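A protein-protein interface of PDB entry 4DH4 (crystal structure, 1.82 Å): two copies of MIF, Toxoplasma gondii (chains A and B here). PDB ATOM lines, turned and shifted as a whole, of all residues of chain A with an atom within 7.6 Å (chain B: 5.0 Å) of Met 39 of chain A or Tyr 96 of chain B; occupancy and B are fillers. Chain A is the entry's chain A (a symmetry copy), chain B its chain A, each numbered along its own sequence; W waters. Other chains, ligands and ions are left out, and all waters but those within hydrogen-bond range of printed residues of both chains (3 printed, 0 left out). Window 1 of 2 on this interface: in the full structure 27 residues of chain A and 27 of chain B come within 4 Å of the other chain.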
ATOM      1  N   PRO A   1     -28.792 -27.636 -18.613  1.00  0.00           N
ATOM      2  CA  PRO A   1     -27.861 -26.989 -17.686  1.00  0.00           C
ATOM      3  C   PRO A   1     -26.475 -27.602 -17.800  1.00  0.00           C
ATOM      4  O   PRO A   1     -26.319 -28.691 -18.354  1.00  0.00           O
ATOM      5  CB  PRO A   1     -28.460 -27.296 -16.306  1.00  0.00           C
ATOM      6  CG  PRO A   1     -29.907 -27.489 -16.559  1.00  0.00           C
ATOM      7  CD  PRO A   1     -30.043 -28.052 -17.955  1.00  0.00           C
ATOM      8  N   LYS A   2     -25.476 -26.901 -17.276  1.00  0.00           N
ATOM      9  CA  LYS A   2     -24.101 -27.371 -17.332  1.00  0.00           C
ATOM     10  C   LYS A   2     -23.435 -27.115 -15.977  1.00  0.00           C
ATOM     11  O   LYS A   2     -23.671 -26.079 -15.344  1.00  0.00           O
ATOM     12  CB  LYS A   2     -23.387 -26.644 -18.468  1.00  0.00           C
ATOM     13  CG  LYS A   2     -21.996 -27.094 -18.787  1.00  0.00           C
ATOM     14  CD  LYS A   2     -21.529 -26.467 -20.098  1.00  0.00           C
ATOM     15  CE  LYS A   2     -21.502 -24.926 -20.030  1.00  0.00           C
ATOM     16  NZ  LYS A   2     -20.358 -24.385 -20.819  1.00  0.00           N
ATOM     17  N   CYS A   3     -22.651 -28.079 -15.513  1.00  0.00           N
ATOM     18  CA  CYS A   3     -21.881 -27.921 -14.285  1.00  0.00           C
ATOM     19  C   CYS A   3     -20.486 -28.500 -14.484  1.00  0.00           C
ATOM     20  O   CYS A   3     -20.337 -29.700 -14.731  1.00  0.00           O
ATOM     21  CB  CYS A   3     -22.582 -28.603 -13.107  1.00  0.00           C
ATOM     22  SG  CYS A   3     -21.566 -28.703 -11.603  1.00  0.00           S
ATOM     23  N   MET A   4     -19.476 -27.642 -14.380  1.00  0.00           N
ATOM     24  CA  MET A   4     -18.090 -28.059 -14.561  1.00  0.00           C
ATOM     25  C   MET A   4     -17.259 -27.740 -13.332  1.00  0.00           C
ATOM     26  O   MET A   4     -17.194 -26.587 -12.898  1.00  0.00           O
ATOM     27  CB  MET A   4     -17.484 -27.399 -15.799  1.00  0.00           C
ATOM     28  CG  MET A   4     -18.125 -27.848 -17.103  1.00  0.00           C
ATOM     29  SD  MET A   4     -17.903 -29.602 -17.455  1.00  0.00           S
ATOM     30  CE  MET A   4     -16.111 -29.734 -17.406  1.00  0.00           C
ATOM     31  N   LEU A  20     -19.946 -36.876  -9.911  1.00  0.00           N
ATOM     32  CA  LEU A  20     -20.722 -36.340 -11.026  1.00  0.00           C
ATOM     33  C   LEU A  20     -22.170 -36.811 -10.996  1.00  0.00           C
ATOM     34  O   LEU A  20     -23.067 -36.074 -11.390  1.00  0.00           O
ATOM     35  CB  LEU A  20     -20.053 -36.629 -12.374  1.00  0.00           C
ATOM     36  CG  LEU A  20     -18.669 -36.012 -12.617  1.00  0.00           C
ATOM     37  CD1 LEU A  20     -18.134 -36.435 -13.975  1.00  0.00           C
ATOM     38  CD2 LEU A  20     -18.671 -34.478 -12.509  1.00  0.00           C
ATOM     39  N   ALA A  23     -23.677 -34.540  -8.537  1.00  0.00           N
ATOM     40  CA  ALA A  23     -23.778 -33.216  -9.157  1.00  0.00           C
ATOM     41  C   ALA A  23     -24.978 -33.106 -10.106  1.00  0.00           C
ATOM     42  O   ALA A  23     -25.759 -32.150 -10.019  1.00  0.00           O
ATOM     43  CB  ALA A  23     -22.489 -32.877  -9.884  1.00  0.00           C
ATOM     44  N   GLU A  24     -25.123 -34.076 -11.008  1.00  0.00           N
ATOM     45  CA  GLU A  24     -26.201 -34.033 -11.992  1.00  0.00           C
ATOM     46  C   GLU A  24     -27.592 -34.037 -11.343  1.00  0.00           C
ATOM     47  O   GLU A  24     -28.488 -33.314 -11.791  1.00  0.00           O
ATOM     48  CB  GLU A  24     -26.042 -35.136 -13.052  1.00  0.00           C
ATOM     49  CG  GLU A  24     -26.220 -36.548 -12.531  1.00  0.00           C
ATOM     50  CD  GLU A  24     -25.796 -37.621 -13.518  1.00  0.00           C
ATOM     51  OE1 GLU A  24     -24.995 -37.335 -14.435  1.00  0.00           O
ATOM     52  OE2 GLU A  24     -26.274 -38.765 -13.364  1.00  0.00           O
ATOM     53  N   VAL A  27     -28.291 -30.547  -9.591  1.00  0.00           N
ATOM     54  CA  VAL A  27     -28.538 -29.492 -10.577  1.00  0.00           C
ATOM     55  C   VAL A  27     -29.939 -29.665 -11.185  1.00  0.00           C
ATOM     56  O   VAL A  27     -30.720 -28.713 -11.229  1.00  0.00           O
ATOM     57  CB  VAL A  27     -27.412 -29.460 -11.659  1.00  0.00           C
ATOM     58  CG1 VAL A  27     -27.802 -28.616 -12.877  1.00  0.00           C
ATOM     59  CG2 VAL A  27     -26.088 -28.969 -11.043  1.00  0.00           C
ATOM     60  N   PRO A  34     -35.111 -31.631 -16.704  1.00  0.00           N
ATOM     61  CA  PRO A  34     -34.904 -33.074 -16.847  1.00  0.00           C
ATOM     62  C   PRO A  34     -33.420 -33.413 -16.845  1.00  0.00           C
ATOM     63  O   PRO A  34     -32.607 -32.661 -17.399  1.00  0.00           O
ATOM     64  CB  PRO A  34     -35.525 -33.398 -18.218  1.00  0.00           C
ATOM     65  CG  PRO A  34     -36.316 -32.193 -18.606  1.00  0.00           C
ATOM     66  CD  PRO A  34     -35.676 -31.028 -17.926  1.00  0.00           C
ATOM     67  N   LEU A  35     -33.073 -34.527 -16.209  1.00  0.00           N
ATOM     68  CA  LEU A  35     -31.701 -35.015 -16.210  1.00  0.00           C
ATOM     69  C   LEU A  35     -31.128 -35.137 -17.631  1.00  0.00           C
ATOM     70  O   LEU A  35     -29.927 -34.929 -17.837  1.00  0.00           O
ATOM     71  CB  LEU A  35     -31.614 -36.346 -15.459  1.00  0.00           C
ATOM     72  CG  LEU A  35     -30.248 -37.031 -15.353  1.00  0.00           C
ATOM     73  CD1 LEU A  35     -29.174 -36.105 -14.779  1.00  0.00           C
ATOM     74  CD2 LEU A  35     -30.370 -38.311 -14.531  1.00  0.00           C
ATOM     75  N   SER A  36     -31.988 -35.428 -18.608  1.00  0.00           N
ATOM     76  CA  SER A  36     -31.562 -35.585 -20.015  1.00  0.00           C
ATOM     77  C   SER A  36     -30.845 -34.358 -20.605  1.00  0.00           C
ATOM     78  O   SER A  36     -30.108 -34.477 -21.595  1.00  0.00           O
ATOM     79  CB  SER A  36     -32.744 -35.979 -20.910  1.00  0.00           C
ATOM     80  OG  SER A  36     -33.749 -34.973 -20.906  1.00  0.00           O
ATOM     81  N   TYR A  37     -31.056 -33.202 -19.978  1.00  0.00           N
ATOM     82  CA  TYR A  37     -30.492 -31.939 -20.452  1.00  0.00           C
ATOM     83  C   TYR A  37     -29.300 -31.469 -19.614  1.00  0.00           C
ATOM     84  O   TYR A  37     -28.687 -30.446 -19.918  1.00  0.00           O
ATOM     85  CB  TYR A  37     -31.579 -30.862 -20.480  1.00  0.00           C
ATOM     86  CG  TYR A  37     -32.638 -31.116 -21.526  1.00  0.00           C
ATOM     87  CD1 TYR A  37     -32.433 -30.739 -22.854  1.00  0.00           C
ATOM     88  CD2 TYR A  37     -33.838 -31.741 -21.192  1.00  0.00           C
ATOM     89  CE1 TYR A  37     -33.401 -30.978 -23.826  1.00  0.00           C
ATOM     90  CE2 TYR A  37     -34.814 -31.982 -22.153  1.00  0.00           C
ATOM     91  CZ  TYR A  37     -34.587 -31.602 -23.467  1.00  0.00           C
ATOM     92  OH  TYR A  37     -35.546 -31.837 -24.428  1.00  0.00           O
ATOM     93  N   VAL A  38     -28.970 -32.227 -18.572  1.00  0.00           N
ATOM     94  CA  VAL A  38     -27.898 -31.837 -17.650  1.00  0.00           C
ATOM     95  C   VAL A  38     -26.551 -32.435 -18.067  1.00  0.00           C
ATOM     96  O   VAL A  38     -26.426 -33.646 -18.216  1.00  0.00           O
ATOM     97  CB  VAL A  38     -28.245 -32.204 -16.186  1.00  0.00           C
ATOM     98  CG1 VAL A  38     -27.086 -31.864 -15.251  1.00  0.00           C
ATOM     99  CG2 VAL A  38     -29.520 -31.468 -15.746  1.00  0.00           C
ATOM    100  N   MET A  39     -25.562 -31.564 -18.267  1.00  0.00           N
ATOM    101  CA  MET A  39     -24.190 -31.974 -18.563  1.00  0.00           C
ATOM    102  C   MET A  39     -23.293 -31.625 -17.381  1.00  0.00           C
ATOM    103  O   MET A  39     -23.358 -30.512 -16.851  1.00  0.00           O
ATOM    104  CB  MET A  39     -23.693 -31.293 -19.844  1.00  0.00           C
ATOM    105  CG  MET A  39     -22.279 -31.714 -20.288  1.00  0.00           C
ATOM    106  SD  MET A  39     -21.773 -31.073 -21.908  1.00  0.00           S
ATOM    107  CE  MET A  39     -22.841 -32.011 -23.016  1.00  0.00           C
ATOM    108  N   VAL A  40     -22.466 -32.582 -16.964  1.00  0.00           N
ATOM    109  CA  VAL A  40     -21.561 -32.392 -15.833  1.00  0.00           C
ATOM    110  C   VAL A  40     -20.155 -32.914 -16.172  1.00  0.00           C
ATOM    111  O   VAL A  40     -20.004 -33.884 -16.927  1.00  0.00           O
ATOM    112  CB  VAL A  40     -22.092 -33.063 -14.521  1.00  0.00           C
ATOM    113  CG1 VAL A  40     -23.326 -32.338 -13.973  1.00  0.00           C
ATOM    114  CG2 VAL A  40     -22.405 -34.553 -14.737  1.00  0.00           C
ATOM    115  N   GLY A  41     -19.130 -32.267 -15.633  1.00  0.00           N
ATOM    116  CA  GLY A  41     -17.770 -32.745 -15.847  1.00  0.00           C
ATOM    117  C   GLY A  41     -16.804 -32.389 -14.740  1.00  0.00           C
ATOM    118  O   GLY A  41     -17.073 -31.508 -13.917  1.00  0.00           O
ATOM    119  N   ARG A  61     -18.286 -24.049 -12.208  1.00  0.00           N
ATOM    120  CA  ARG A  61     -19.057 -23.145 -13.056  1.00  0.00           C
ATOM    121  C   ARG A  61     -20.378 -23.797 -13.392  1.00  0.00           C
ATOM    122  O   ARG A  61     -20.397 -24.895 -13.961  1.00  0.00           O
ATOM    123  CB  ARG A  61     -18.304 -22.834 -14.358  1.00  0.00           C
ATOM    124  CG  ARG A  61     -16.936 -22.187 -14.190  1.00  0.00           C
ATOM    125  CD  ARG A  61     -16.453 -21.622 -15.528  1.00  0.00           C
ATOM    126  NE  ARG A  61     -17.266 -20.475 -15.937  1.00  0.00           N
ATOM    127  CZ  ARG A  61     -18.048 -20.444 -17.012  1.00  0.00           C
ATOM    128  NH1 ARG A  61     -18.116 -21.494 -17.832  1.00  0.00           N
ATOM    129  NH2 ARG A  61     -18.752 -19.352 -17.277  1.00  0.00           N
ATOM    130  N   ALA A  63     -24.150 -23.167 -15.373  1.00  0.00           N
ATOM    131  CA  ALA A  63     -24.892 -22.358 -16.355  1.00  0.00           C
ATOM    132  C   ALA A  63     -26.241 -22.993 -16.640  1.00  0.00           C
ATOM    133  O   ALA A  63     -26.368 -24.215 -16.655  1.00  0.00           O
ATOM    134  CB  ALA A  63     -24.101 -22.242 -17.661  1.00  0.00           C
ATOM    135  N   ILE A  65     -30.262 -22.081 -18.822  1.00  0.00           N
ATOM    136  CA  ILE A  65     -31.182 -21.184 -19.520  1.00  0.00           C
ATOM    137  C   ILE A  65     -32.299 -20.881 -18.537  1.00  0.00           C
ATOM    138  O   ILE A  65     -33.212 -21.687 -18.343  1.00  0.00           O
ATOM    139  CB  ILE A  65     -31.749 -21.808 -20.810  1.00  0.00           C
ATOM    140  CG1 ILE A  65     -30.610 -22.238 -21.741  1.00  0.00           C
ATOM    141  CG2 ILE A  65     -32.700 -20.814 -21.516  1.00  0.00           C
ATOM    142  CD1 ILE A  65     -31.038 -23.249 -22.810  1.00  0.00           C
ATOM    143  N   TRP A 107     -27.375 -20.981 -26.504  1.00  0.00           N
ATOM    144  CA  TRP A 107     -27.130 -22.364 -26.118  1.00  0.00           C
ATOM    145  C   TRP A 107     -27.551 -23.289 -27.251  1.00  0.00           C
ATOM    146  O   TRP A 107     -28.695 -23.232 -27.716  1.00  0.00           O
ATOM    147  CB  TRP A 107     -27.911 -22.691 -24.840  1.00  0.00           C
ATOM    148  CG  TRP A 107     -27.383 -23.869 -24.050  1.00  0.00           C
ATOM    149  CD1 TRP A 107     -27.156 -25.140 -24.506  1.00  0.00           C
ATOM    150  CD2 TRP A 107     -27.062 -23.883 -22.653  1.00  0.00           C
ATOM    151  NE1 TRP A 107     -26.689 -25.935 -23.479  1.00  0.00           N
ATOM    152  CE2 TRP A 107     -26.626 -25.188 -22.333  1.00  0.00           C
ATOM    153  CE3 TRP A 107     -27.079 -22.910 -21.644  1.00  0.00           C
ATOM    154  CZ2 TRP A 107     -26.219 -25.550 -21.037  1.00  0.00           C
ATOM    155  CZ3 TRP A 107     -26.679 -23.270 -20.356  1.00  0.00           C
ATOM    156  CH2 TRP A 107     -26.256 -24.579 -20.066  1.00  0.00           C
ATOM    157  N   ALA A 108     -26.611 -24.116 -27.709  1.00  0.00           N
ATOM    158  CA  ALA A 108     -26.869 -25.077 -28.778  1.00  0.00           C
ATOM    159  C   ALA A 108     -26.633 -26.516 -28.323  1.00  0.00           C
ATOM    160  O   ALA A 108     -25.777 -26.786 -27.489  1.00  0.00           O
ATOM    161  CB  ALA A 108     -25.991 -24.768 -29.983  1.00  0.00           C
ATOM    162  N   MET A 109     -27.423 -27.433 -28.870  1.00  0.00           N
ATOM    163  CA  MET A 109     -27.151 -28.861 -28.742  1.00  0.00           C
ATOM    164  C   MET A 109     -27.038 -29.395 -30.160  1.00  0.00           C
ATOM    165  O   MET A 109     -27.966 -29.256 -30.966  1.00  0.00           O
ATOM    166  CB  MET A 109     -28.262 -29.567 -27.964  1.00  0.00           C
ATOM    167  CG  MET A 109     -27.949 -31.018 -27.602  1.00  0.00           C
ATOM    168  SD  MET A 109     -29.299 -31.823 -26.718  1.00  0.00           S
ATOM    169  CE  MET A 109     -30.472 -32.034 -28.055  1.00  0.00           C
ATOM    170  N   GLY A 110     -25.873 -29.952 -30.485  1.00  0.00           N
ATOM    171  CA  GLY A 110     -25.568 -30.267 -31.876  1.00  0.00           C
ATOM    172  C   GLY A 110     -25.714 -29.038 -32.762  1.00  0.00           C
ATOM    173  O   GLY A 110     -25.131 -27.988 -32.486  1.00  0.00           O
ATOM    174  N   ARG A 112     -28.428 -27.202 -33.435  1.00  0.00           N
ATOM    175  CA  ARG A 112     -29.650 -26.447 -33.138  1.00  0.00           C
ATOM    176  C   ARG A 112     -29.492 -25.619 -31.857  1.00  0.00           C
ATOM    177  O   ARG A 112     -28.985 -26.121 -30.857  1.00  0.00           O
ATOM    178  CB  ARG A 112     -30.839 -27.404 -32.982  1.00  0.00           C
ATOM    179  CG  ARG A 112     -31.060 -28.348 -34.171  1.00  0.00           C
ATOM    180  CD  ARG A 112     -32.230 -29.304 -33.955  1.00  0.00           C
ATOM    181  NE  ARG A 112     -31.975 -30.267 -32.882  1.00  0.00           N
ATOM    182  CZ  ARG A 112     -32.821 -31.224 -32.507  1.00  0.00           C
ATOM    183  NH1 ARG A 112     -33.993 -31.371 -33.120  1.00  0.00           N
ATOM    184  NH2 ARG A 112     -32.491 -32.044 -31.518  1.00  0.00           N
ATOM    185  N   PHE A 114     -31.431 -23.490 -28.683  1.00  0.00           N
ATOM    186  CA  PHE A 114     -32.659 -23.617 -27.908  1.00  0.00           C
ATOM    187  C   PHE A 114     -33.624 -22.460 -28.153  1.00  0.00           C
ATOM    188  O   PHE A 114     -33.305 -21.467 -28.812  1.00  0.00           O
ATOM    189  CB  PHE A 114     -32.341 -23.738 -26.415  1.00  0.00           C
ATOM    190  CG  PHE A 114     -31.886 -25.104 -26.009  1.00  0.00           C
ATOM    191  CD1 PHE A 114     -30.531 -25.409 -25.941  1.00  0.00           C
ATOM    192  CD2 PHE A 114     -32.814 -26.092 -25.699  1.00  0.00           C
ATOM    193  CE1 PHE A 114     -30.104 -26.679 -25.566  1.00  0.00           C
ATOM    194  CE2 PHE A 114     -32.401 -27.364 -25.332  1.00  0.00           C
ATOM    195  CZ  PHE A 114     -31.041 -27.659 -25.259  1.00  0.00           C
ATOM    196  OXT PHE A 114     -34.762 -22.502 -27.684  1.00  0.00           O
ATOM    197  N   MET B  48     -16.881 -36.939 -18.021  1.00  0.00           N
ATOM    198  CA  MET B  48     -18.018 -36.081 -18.328  1.00  0.00           C
ATOM    199  C   MET B  48     -19.264 -36.938 -18.509  1.00  0.00           C
ATOM    200  O   MET B  48     -19.196 -38.046 -19.061  1.00  0.00           O
ATOM    201  CB  MET B  48     -17.745 -35.236 -19.578  1.00  0.00           C
ATOM    202  CG  MET B  48     -16.920 -33.966 -19.311  1.00  0.00           C
ATOM    203  SD  MET B  48     -16.689 -32.899 -20.765  1.00  0.00           S
ATOM    204  CE  MET B  48     -18.371 -32.701 -21.316  1.00  0.00           C
ATOM    205  N   ARG B  49     -20.390 -36.438 -18.013  1.00  0.00           N
ATOM    206  CA  ARG B  49     -21.679 -37.095 -18.191  1.00  0.00           C
ATOM    207  C   ARG B  49     -22.670 -36.132 -18.830  1.00  0.00           C
ATOM    208  O   ARG B  49     -22.595 -34.919 -18.616  1.00  0.00           O
ATOM    209  CB  ARG B  49     -22.232 -37.586 -16.851  1.00  0.00           C
ATOM    210  CG  ARG B  49     -21.402 -38.703 -16.208  1.00  0.00           C
ATOM    211  CD  ARG B  49     -21.826 -38.965 -14.775  1.00  0.00           C
ATOM    212  NE  ARG B  49     -23.199 -39.452 -14.675  1.00  0.00           N
ATOM    213  CZ  ARG B  49     -23.571 -40.714 -14.878  1.00  0.00           C
ATOM    214  NH1 ARG B  49     -24.845 -41.050 -14.758  1.00  0.00           N
ATOM    215  NH2 ARG B  49     -22.673 -41.643 -15.201  1.00  0.00           N
ATOM    216  N   PHE B  50     -23.588 -36.680 -19.618  1.00  0.00           N
ATOM    217  CA  PHE B  50     -24.664 -35.899 -20.222  1.00  0.00           C
ATOM    218  C   PHE B  50     -25.912 -36.759 -20.303  1.00  0.00           C
ATOM    219  O   PHE B  50     -25.862 -37.895 -20.779  1.00  0.00           O
ATOM    220  CB  PHE B  50     -24.256 -35.362 -21.606  1.00  0.00           C
ATOM    221  CG  PHE B  50     -25.328 -34.543 -22.300  1.00  0.00           C
ATOM    222  CD1 PHE B  50     -26.049 -33.567 -21.607  1.00  0.00           C
ATOM    223  CD2 PHE B  50     -25.586 -34.726 -23.656  1.00  0.00           C
ATOM    224  CE1 PHE B  50     -27.037 -32.806 -22.247  1.00  0.00           C
ATOM    225  CE2 PHE B  50     -26.571 -33.967 -24.316  1.00  0.00           C
ATOM    226  CZ  PHE B  50     -27.298 -33.002 -23.600  1.00  0.00           C
ATOM    227  N   CYS B  57     -19.339 -37.222 -24.747  1.00  0.00           N
ATOM    228  CA  CYS B  57     -20.050 -35.965 -24.910  1.00  0.00           C
ATOM    229  C   CYS B  57     -18.990 -34.871 -24.900  1.00  0.00           C
ATOM    230  O   CYS B  57     -17.814 -35.142 -24.640  1.00  0.00           O
ATOM    231  CB  CYS B  57     -21.061 -35.766 -23.769  1.00  0.00           C
ATOM    232  SG  CYS B  57     -20.345 -35.553 -22.113  1.00  0.00           S
ATOM    233  N   ALA B  58     -19.390 -33.643 -25.202  1.00  0.00           N
ATOM    234  CA  ALA B  58     -18.459 -32.526 -25.178  1.00  0.00           C
ATOM    235  C   ALA B  58     -19.200 -31.238 -24.894  1.00  0.00           C
ATOM    236  O   ALA B  58     -20.414 -31.143 -25.100  1.00  0.00           O
ATOM    237  CB  ALA B  58     -17.707 -32.421 -26.506  1.00  0.00           C
ATOM    238  N   PHE B  59     -18.470 -30.250 -24.399  1.00  0.00           N
ATOM    239  CA  PHE B  59     -19.008 -28.906 -24.412  1.00  0.00           C
ATOM    240  C   PHE B  59     -17.977 -27.921 -24.906  1.00  0.00           C
ATOM    241  O   PHE B  59     -16.767 -28.071 -24.671  1.00  0.00           O
ATOM    242  CB  PHE B  59     -19.641 -28.509 -23.081  1.00  0.00           C
ATOM    243  CG  PHE B  59     -18.670 -28.037 -22.072  1.00  0.00           C
ATOM    244  CD1 PHE B  59     -17.930 -28.940 -21.332  1.00  0.00           C
ATOM    245  CD2 PHE B  59     -18.485 -26.681 -21.861  1.00  0.00           C
ATOM    246  CE1 PHE B  59     -17.017 -28.487 -20.399  1.00  0.00           C
ATOM    247  CE2 PHE B  59     -17.582 -26.222 -20.930  1.00  0.00           C
ATOM    248  CZ  PHE B  59     -16.848 -27.126 -20.189  1.00  0.00           C
ATOM    249  N   ILE B  60     -18.441 -26.928 -25.647  1.00  0.00           N
ATOM    250  CA  ILE B  60     -17.517 -25.942 -26.167  1.00  0.00           C
ATOM    251  C   ILE B  60     -18.022 -24.542 -25.841  1.00  0.00           C
ATOM    252  O   ILE B  60     -19.226 -24.267 -25.890  1.00  0.00           O
ATOM    253  CB  ILE B  60     -17.158 -26.167 -27.688  1.00  0.00           C
ATOM    254  CG1 ILE B  60     -17.969 -25.279 -28.627  1.00  0.00           C
ATOM    255  CG2 ILE B  60     -17.252 -27.647 -28.098  1.00  0.00           C
ATOM    256  CD1 ILE B  60     -17.323 -23.954 -28.892  1.00  0.00           C
ATOM    257  N   ARG B  94     -24.710 -34.920 -28.606  1.00  0.00           N
ATOM    258  CA  ARG B  94     -24.162 -34.945 -27.247  1.00  0.00           C
ATOM    259  C   ARG B  94     -23.118 -33.845 -27.038  1.00  0.00           C
ATOM    260  O   ARG B  94     -22.275 -33.932 -26.156  1.00  0.00           O
ATOM    261  CB  ARG B  94     -23.612 -36.332 -26.896  1.00  0.00           C
ATOM    262  CG  ARG B  94     -24.741 -37.335 -26.662  1.00  0.00           C
ATOM    263  CD  ARG B  94     -24.268 -38.716 -26.270  1.00  0.00           C
ATOM    264  NE  ARG B  94     -23.605 -38.792 -24.968  1.00  0.00           N
ATOM    265  CZ  ARG B  94     -24.214 -38.721 -23.782  1.00  0.00           C
ATOM    266  NH1 ARG B  94     -25.528 -38.526 -23.689  1.00  0.00           N
ATOM    267  NH2 ARG B  94     -23.495 -38.841 -22.677  1.00  0.00           N
ATOM    268  N   ILE B  95     -23.213 -32.797 -27.853  1.00  0.00           N
ATOM    269  CA  ILE B  95     -22.317 -31.650 -27.747  1.00  0.00           C
ATOM    270  C   ILE B  95     -23.111 -30.393 -27.450  1.00  0.00           C
ATOM    271  O   ILE B  95     -24.034 -30.041 -28.203  1.00  0.00           O
ATOM    272  CB  ILE B  95     -21.491 -31.458 -29.042  1.00  0.00           C
ATOM    273  CG1 ILE B  95     -20.650 -32.704 -29.309  1.00  0.00           C
ATOM    274  CG2 ILE B  95     -20.602 -30.192 -28.954  1.00  0.00           C
ATOM    275  CD1 ILE B  95     -20.040 -32.745 -30.690  1.00  0.00           C
ATOM    276  N   TYR B  96     -22.772 -29.748 -26.330  1.00  0.00           N
ATOM    277  CA  TYR B  96     -23.321 -28.436 -25.993  1.00  0.00           C
ATOM    278  C   TYR B  96     -22.334 -27.363 -26.406  1.00  0.00           C
ATOM    279  O   TYR B  96     -21.150 -27.444 -26.074  1.00  0.00           O
ATOM    280  CB  TYR B  96     -23.567 -28.289 -24.490  1.00  0.00           C
ATOM    281  CG  TYR B  96     -24.927 -28.724 -23.964  1.00  0.00           C
ATOM    282  CD1 TYR B  96     -26.021 -28.931 -24.822  1.00  0.00           C
ATOM    283  CD2 TYR B  96     -25.126 -28.881 -22.585  1.00  0.00           C
ATOM    284  CE1 TYR B  96     -27.270 -29.322 -24.313  1.00  0.00           C
ATOM    285  CE2 TYR B  96     -26.366 -29.260 -22.069  1.00  0.00           C
ATOM    286  CZ  TYR B  96     -27.432 -29.475 -22.939  1.00  0.00           C
ATOM    287  OH  TYR B  96     -28.664 -29.850 -22.431  1.00  0.00           O
ATOM    288  N   THR B  97     -22.824 -26.359 -27.125  1.00  0.00           N
ATOM    289  CA  THR B  97     -22.032 -25.170 -27.433  1.00  0.00           C
ATOM    290  C   THR B  97     -22.752 -23.966 -26.834  1.00  0.00           C
ATOM    291  O   THR B  97     -23.940 -23.770 -27.093  1.00  0.00           O
ATOM    292  CB  THR B  97     -21.847 -24.977 -28.958  1.00  0.00           C
ATOM    293  OG1 THR B  97     -21.279 -26.158 -29.542  1.00  0.00           O
ATOM    294  CG2 THR B  97     -20.916 -23.809 -29.233  1.00  0.00           C
ATOM    295  N   THR B  98     -22.046 -23.188 -26.014  1.00  0.00           N
ATOM    296  CA  THR B  98     -22.628 -21.966 -25.438  1.00  0.00           C
ATOM    297  C   THR B  98     -21.836 -20.743 -25.861  1.00  0.00           C
ATOM    298  O   THR B  98     -20.613 -20.812 -26.061  1.00  0.00           O
ATOM    299  CB  THR B  98     -22.772 -22.030 -23.893  1.00  0.00           C
ATOM    300  OG1 THR B  98     -21.478 -22.050 -23.274  1.00  0.00           O
ATOM    301  CG2 THR B  98     -23.565 -23.262 -23.469  1.00  0.00           C
HETATM  302  O   HOH W   1     -25.566 -36.168 -16.859  1.00  0.00           O
HETATM  303  O   HOH W   2     -23.501 -27.771 -30.202  1.00  0.00           O
HETATM  304  O   HOH W   3     -20.396 -24.621 -23.447  1.00  0.00           O
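Water W1 lies within hydrogen-bond range of the side-chain carboxylate of Glu 24 of chain A (2.8 Å), the backbone carbonyl oxygen of Val 38 of chain A (3.0 Å) and the backbone NH of Phe 50 of chain B (3.4 Å).
Printed residues of chain B that touch a printed residue of chain A: Met 48, Arg 49, Phe 50, Ala 58, Phe 59, Arg 94, Ile 95, Tyr 96, Thr 97 and Thr 98.
Hydrophobic or aromatic side chains of chain B within 4 Å of the printed part of chain A: Met 48, Phe 50, Phe 59 and Tyr 96.
Along chain A the printed residues that touch a printed residue of chain B span positions 1 to 110.
Among the printed residues, Asp or Glu carboxylates within 4 Å of a Lys or Arg side-chain nitrogen of the other chain: Glu 24 of chain A with Arg 49 of chain B (2.8 Å).
OH of Tyr 96 of chain B lies within hydrogen-bond range of O of Tyr 37 of chain A, 2.6 Å away.
The backbone carbonyl oxygen (O) of Ala 58 of chain B lies close to the side-chain sulfur (SD) of Met 39 of chain A (3.5 Å).
The guanidinium group (NE) of Arg 49 of chain B lies within salt-bridge range of the side-chain carboxylate (OE1) of Glu 24 of chain A, 2.8 Å away.
The backbone NH of Arg 49 of chain B lies within hydrogen-bond range of the backbone carbonyl oxygen of Val 40 of chain A, at 2.8 Å.
O of Ile 95 of chain B lies within hydrogen-bond range of N of Gly 110 of chain A (2.9 Å).
O of Thr 97 of chain B lies within hydrogen-bond range of N of Ala 108 of chain A (2.8 Å).
No position is printed for both chains.
Of the 30 pairs that touch across the chains among the printed residues, none has its exchanged pair printed and touching as well.
The backbone NH (N) of Ile 60 of chain B lies within hydrogen-bond range of the backbone carbonyl oxygen (O) of Tyr 96 of chain B (2.8 Å).
O of Cys 3 of chain A sits at hydrogen-bond distance from N of Gly 41 of chain A, 3.0 Å away.
Of the printed residues of chain B, Gly 110 of chain A touches Ile 95 (2.9 Å).
Of the printed residues of chain A, Tyr 96 of chain B touches Pro 1, Tyr 37, Met 39, Trp 107, Ala 108 and Met 109.
The nearest printed residue of chain A that does not touch Tyr 96 of chain B is Phe 114 of chain A (4.1 Å).
The nearest printed residue of chain A that does not touch Arg 49 of chain B is Val 38 of chain A (4.1 Å).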
